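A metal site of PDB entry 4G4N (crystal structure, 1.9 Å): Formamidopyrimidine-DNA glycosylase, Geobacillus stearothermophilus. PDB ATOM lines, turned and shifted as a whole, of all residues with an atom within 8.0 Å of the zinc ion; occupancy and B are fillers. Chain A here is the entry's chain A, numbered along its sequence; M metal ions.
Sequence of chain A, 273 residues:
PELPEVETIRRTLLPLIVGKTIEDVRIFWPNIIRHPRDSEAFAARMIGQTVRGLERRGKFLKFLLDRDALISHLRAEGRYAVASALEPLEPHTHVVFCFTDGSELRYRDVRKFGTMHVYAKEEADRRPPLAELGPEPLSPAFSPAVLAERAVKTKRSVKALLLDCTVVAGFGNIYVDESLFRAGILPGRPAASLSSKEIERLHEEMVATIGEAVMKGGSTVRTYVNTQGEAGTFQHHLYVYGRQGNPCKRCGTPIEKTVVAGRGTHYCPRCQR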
ATOM      1  N   PHE A 181     -23.425  -4.304  35.387  1.00  0.00           N
ATOM      2  CA  PHE A 181     -24.526  -3.537  34.833  1.00  0.00           C
ATOM      3  C   PHE A 181     -25.790  -3.682  35.680  1.00  0.00           C
ATOM      4  O   PHE A 181     -26.455  -2.689  36.016  1.00  0.00           O
ATOM      5  CB  PHE A 181     -24.847  -3.950  33.398  1.00  0.00           C
ATOM      6  CG  PHE A 181     -26.137  -3.358  32.903  1.00  0.00           C
ATOM      7  CD1 PHE A 181     -26.167  -2.070  32.405  1.00  0.00           C
ATOM      8  CD2 PHE A 181     -27.324  -4.062  33.023  1.00  0.00           C
ATOM      9  CE1 PHE A 181     -27.366  -1.496  31.983  1.00  0.00           C
ATOM     10  CE2 PHE A 181     -28.523  -3.504  32.596  1.00  0.00           C
ATOM     11  CZ  PHE A 181     -28.543  -2.204  32.081  1.00  0.00           C
ATOM     12  N   TYR A 239     -27.367  -7.682  28.577  1.00  0.00           N
ATOM     13  CA  TYR A 239     -27.596  -6.239  28.670  1.00  0.00           C
ATOM     14  C   TYR A 239     -26.453  -5.465  28.056  1.00  0.00           C
ATOM     15  O   TYR A 239     -26.665  -4.411  27.440  1.00  0.00           O
ATOM     16  CB  TYR A 239     -27.740  -5.828  30.138  1.00  0.00           C
ATOM     17  CG  TYR A 239     -29.042  -6.261  30.748  1.00  0.00           C
ATOM     18  CD1 TYR A 239     -29.092  -7.332  31.654  1.00  0.00           C
ATOM     19  CD2 TYR A 239     -30.226  -5.631  30.418  1.00  0.00           C
ATOM     20  CE1 TYR A 239     -30.288  -7.739  32.214  1.00  0.00           C
ATOM     21  CE2 TYR A 239     -31.428  -6.034  30.966  1.00  0.00           C
ATOM     22  CZ  TYR A 239     -31.455  -7.077  31.862  1.00  0.00           C
ATOM     23  OH  TYR A 239     -32.663  -7.459  32.403  1.00  0.00           O
ATOM     24  N   VAL A 240     -25.229  -5.942  28.244  1.00  0.00           N
ATOM     25  CA  VAL A 240     -24.088  -5.146  27.809  1.00  0.00           C
ATOM     26  C   VAL A 240     -23.034  -5.914  27.042  1.00  0.00           C
ATOM     27  O   VAL A 240     -22.424  -5.384  26.115  1.00  0.00           O
ATOM     28  CB  VAL A 240     -23.425  -4.374  28.984  1.00  0.00           C
ATOM     29  CG1 VAL A 240     -24.416  -3.384  29.604  1.00  0.00           C
ATOM     30  CG2 VAL A 240     -22.876  -5.356  30.041  1.00  0.00           C
ATOM     31  N   PRO A 247     -28.195   0.296  21.744  1.00  0.00           N
ATOM     32  CA  PRO A 247     -28.859   0.964  22.864  1.00  0.00           C
ATOM     33  C   PRO A 247     -28.989   0.054  24.070  1.00  0.00           C
ATOM     34  O   PRO A 247     -29.295  -1.145  23.942  1.00  0.00           O
ATOM     35  CB  PRO A 247     -30.277   1.245  22.323  1.00  0.00           C
ATOM     36  CG  PRO A 247     -30.155   1.115  20.824  1.00  0.00           C
ATOM     37  CD  PRO A 247     -29.113   0.076  20.611  1.00  0.00           C
ATOM     38  N   CYS A 248     -28.746   0.620  25.249  1.00  0.00           N
ATOM     39  CA  CYS A 248     -29.035  -0.050  26.501  1.00  0.00           C
ATOM     40  C   CYS A 248     -30.492  -0.490  26.499  1.00  0.00           C
ATOM     41  O   CYS A 248     -31.379   0.248  26.070  1.00  0.00           O
ATOM     42  CB  CYS A 248     -28.778   0.900  27.672  1.00  0.00           C
ATOM     43  SG  CYS A 248     -29.188   0.190  29.286  1.00  0.00           S
ATOM     44  N   LYS A 249     -30.742  -1.719  26.969  1.00  0.00           N
ATOM     45  CA  LYS A 249     -32.095  -2.251  27.026  1.00  0.00           C
ATOM     46  C   LYS A 249     -32.937  -1.638  28.133  1.00  0.00           C
ATOM     47  O   LYS A 249     -34.167  -1.812  28.148  1.00  0.00           O
ATOM     48  CB  LYS A 249     -32.042  -3.780  27.193  1.00  0.00           C
ATOM     49  CG  LYS A 249     -31.340  -4.480  26.037  1.00  0.00           C
ATOM     50  CD  LYS A 249     -31.453  -6.004  26.153  1.00  0.00           C
ATOM     51  CE  LYS A 249     -30.918  -6.689  24.893  1.00  0.00           C
ATOM     52  NZ  LYS A 249     -30.987  -8.182  25.007  1.00  0.00           N
ATOM     53  N   ARG A 250     -32.297  -0.931  29.070  1.00  0.00           N
ATOM     54  CA  ARG A 250     -33.004  -0.295  30.176  1.00  0.00           C
ATOM     55  C   ARG A 250     -33.237   1.198  29.954  1.00  0.00           C
ATOM     56  O   ARG A 250     -34.260   1.738  30.373  1.00  0.00           O
ATOM     57  CB  ARG A 250     -32.246  -0.495  31.495  1.00  0.00           C
ATOM     58  CG  ARG A 250     -32.176  -1.933  31.968  1.00  0.00           C
ATOM     59  CD  ARG A 250     -33.262  -2.250  32.976  1.00  0.00           C
ATOM     60  NE  ARG A 250     -33.184  -3.626  33.464  1.00  0.00           N
ATOM     61  CZ  ARG A 250     -32.403  -4.018  34.468  1.00  0.00           C
ATOM     62  NH1 ARG A 250     -32.389  -5.285  34.841  1.00  0.00           N
ATOM     63  NH2 ARG A 250     -31.629  -3.138  35.104  1.00  0.00           N
ATOM     64  N   CYS A 251     -32.280   1.872  29.315  1.00  0.00           N
ATOM     65  CA  CYS A 251     -32.402   3.327  29.174  1.00  0.00           C
ATOM     66  C   CYS A 251     -32.167   3.868  27.777  1.00  0.00           C
ATOM     67  O   CYS A 251     -32.367   5.057  27.540  1.00  0.00           O
ATOM     68  CB  CYS A 251     -31.451   4.048  30.139  1.00  0.00           C
ATOM     69  SG  CYS A 251     -29.710   3.996  29.582  1.00  0.00           S
ATOM     70  N   GLY A 252     -31.692   3.022  26.860  1.00  0.00           N
ATOM     71  CA  GLY A 252     -31.512   3.421  25.469  1.00  0.00           C
ATOM     72  C   GLY A 252     -30.198   4.117  25.123  1.00  0.00           C
ATOM     73  O   GLY A 252     -29.923   4.385  23.955  1.00  0.00           O
ATOM     74  N   THR A 253     -29.395   4.411  26.138  1.00  0.00           N
ATOM     75  CA  THR A 253     -28.084   5.022  25.946  1.00  0.00           C
ATOM     76  C   THR A 253     -27.159   4.015  25.262  1.00  0.00           C
ATOM     77  O   THR A 253     -27.175   2.842  25.607  1.00  0.00           O
ATOM     78  CB  THR A 253     -27.467   5.393  27.317  1.00  0.00           C
ATOM     79  OG1 THR A 253     -28.269   6.389  27.972  1.00  0.00           O
ATOM     80  CG2 THR A 253     -26.040   5.930  27.145  1.00  0.00           C
ATOM     81  N   PRO A 254     -26.349   4.463  24.287  1.00  0.00           N
ATOM     82  CA  PRO A 254     -25.484   3.459  23.633  1.00  0.00           C
ATOM     83  C   PRO A 254     -24.496   2.805  24.602  1.00  0.00           C
ATOM     84  O   PRO A 254     -23.851   3.471  25.402  1.00  0.00           O
ATOM     85  CB  PRO A 254     -24.725   4.282  22.581  1.00  0.00           C
ATOM     86  CG  PRO A 254     -25.645   5.439  22.285  1.00  0.00           C
ATOM     87  CD  PRO A 254     -26.244   5.778  23.644  1.00  0.00           C
ATOM     88  N   ILE A 255     -24.405   1.483  24.515  1.00  0.00           N
ATOM     89  CA  ILE A 255     -23.470   0.740  25.342  1.00  0.00           C
ATOM     90  C   ILE A 255     -22.060   1.052  24.886  1.00  0.00           C
ATOM     91  O   ILE A 255     -21.815   1.173  23.686  1.00  0.00           O
ATOM     92  CB  ILE A 255     -23.756  -0.765  25.262  1.00  0.00           C
ATOM     93  CG1 ILE A 255     -25.143  -1.035  25.858  1.00  0.00           C
ATOM     94  CG2 ILE A 255     -22.627  -1.593  25.954  1.00  0.00           C
ATOM     95  CD1 ILE A 255     -25.344  -0.379  27.260  1.00  0.00           C
ATOM     96  N   TYR A 267     -20.334  -1.549  29.187  1.00  0.00           N
ATOM     97  CA  TYR A 267     -21.136  -0.943  30.239  1.00  0.00           C
ATOM     98  C   TYR A 267     -22.055   0.143  29.667  1.00  0.00           C
ATOM     99  O   TYR A 267     -21.821   0.661  28.572  1.00  0.00           O
ATOM    100  CB  TYR A 267     -20.236  -0.343  31.320  1.00  0.00           C
ATOM    101  CG  TYR A 267     -19.316   0.719  30.756  1.00  0.00           C
ATOM    102  CD1 TYR A 267     -19.671   2.058  30.795  1.00  0.00           C
ATOM    103  CD2 TYR A 267     -18.111   0.387  30.137  1.00  0.00           C
ATOM    104  CE1 TYR A 267     -18.856   3.044  30.265  1.00  0.00           C
ATOM    105  CE2 TYR A 267     -17.281   1.363  29.597  1.00  0.00           C
ATOM    106  CZ  TYR A 267     -17.661   2.692  29.669  1.00  0.00           C
ATOM    107  OH  TYR A 267     -16.860   3.687  29.148  1.00  0.00           O
ATOM    108  N   CYS A 268     -23.096   0.453  30.429  1.00  0.00           N
ATOM    109  CA  CYS A 268     -23.938   1.611  30.129  1.00  0.00           C
ATOM    110  C   CYS A 268     -23.490   2.773  31.008  1.00  0.00           C
ATOM    111  O   CYS A 268     -23.544   2.682  32.242  1.00  0.00           O
ATOM    112  CB  CYS A 268     -25.404   1.288  30.412  1.00  0.00           C
ATOM    113  SG  CYS A 268     -26.426   2.766  30.192  1.00  0.00           S
ATOM    114  N   PRO A 269     -23.046   3.867  30.387  1.00  0.00           N
ATOM    115  CA  PRO A 269     -22.534   4.991  31.176  1.00  0.00           C
ATOM    116  C   PRO A 269     -23.633   5.772  31.904  1.00  0.00           C
ATOM    117  O   PRO A 269     -23.317   6.642  32.713  1.00  0.00           O
ATOM    118  CB  PRO A 269     -21.837   5.861  30.128  1.00  0.00           C
ATOM    119  CG  PRO A 269     -22.640   5.629  28.897  1.00  0.00           C
ATOM    120  CD  PRO A 269     -23.000   4.152  28.942  1.00  0.00           C
ATOM    121  N   ARG A 270     -24.907   5.464  31.653  1.00  0.00           N
ATOM    122  CA  ARG A 270     -26.007   6.104  32.409  1.00  0.00           C
ATOM    123  C   ARG A 270     -26.481   5.250  33.593  1.00  0.00           C
ATOM    124  O   ARG A 270     -26.640   5.752  34.714  1.00  0.00           O
ATOM    125  CB  ARG A 270     -27.190   6.411  31.488  1.00  0.00           C
ATOM    126  CG  ARG A 270     -28.373   7.036  32.214  1.00  0.00           C
ATOM    127  CD  ARG A 270     -29.515   7.427  31.276  1.00  0.00           C
ATOM    128  NE  ARG A 270     -30.613   7.989  32.047  1.00  0.00           N
ATOM    129  CZ  ARG A 270     -31.728   8.488  31.537  1.00  0.00           C
ATOM    130  NH1 ARG A 270     -32.654   8.992  32.356  1.00  0.00           N
ATOM    131  NH2 ARG A 270     -31.932   8.484  30.225  1.00  0.00           N
ATOM    132  N   CYS A 271     -26.735   3.971  33.333  1.00  0.00           N
ATOM    133  CA  CYS A 271     -27.240   3.040  34.360  1.00  0.00           C
ATOM    134  C   CYS A 271     -26.176   2.729  35.410  1.00  0.00           C
ATOM    135  O   CYS A 271     -26.499   2.441  36.545  1.00  0.00           O
ATOM    136  CB  CYS A 271     -27.703   1.716  33.729  1.00  0.00           C
ATOM    137  SG  CYS A 271     -29.284   1.790  32.727  1.00  0.00           S
ATOM    138  N   GLN A 272     -24.908   2.754  35.003  1.00  0.00           N
ATOM    139  CA  GLN A 272     -23.834   2.397  35.928  1.00  0.00           C
ATOM    140  C   GLN A 272     -23.067   3.626  36.376  1.00  0.00           C
ATOM    141  O   GLN A 272     -22.748   4.494  35.572  1.00  0.00           O
ATOM    142  CB  GLN A 272     -22.877   1.387  35.277  1.00  0.00           C
ATOM    143  CG  GLN A 272     -23.549   0.061  34.980  1.00  0.00           C
ATOM    144  CD  GLN A 272     -22.733  -0.822  34.061  1.00  0.00           C
ATOM    145  OE1 GLN A 272     -23.062  -0.977  32.882  1.00  0.00           O
ATOM    146  NE2 GLN A 272     -21.666  -1.417  34.588  1.00  0.00           N
HETATM  147 ZN    ZN M   1     -28.631   2.127  30.506  1.00  0.00          ZN
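Of the 18 residues printed, 4 come within 4 Å of the zinc ion.
The side-chain sulfur of Cys 251 sits close to the side-chain hydroxyl of Thr 253, 3.2 Å away.
N of Cys 248 sits at hydrogen-bond distance from O of Thr 253 (2.7 Å).
OE1 of Gln 272 is in hydrogen-bond range of N of Cys 268, at 2.8 Å.
N of Arg 270 sits close to SG of Cys 268 (3.4 Å).
N of Arg 250 sits close to SG of Cys 248 (3.3 Å).
The zinc ion is bound by SG of Cys 268, SG of Cys 271, SG of Cys 251 and SG of Cys 248.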
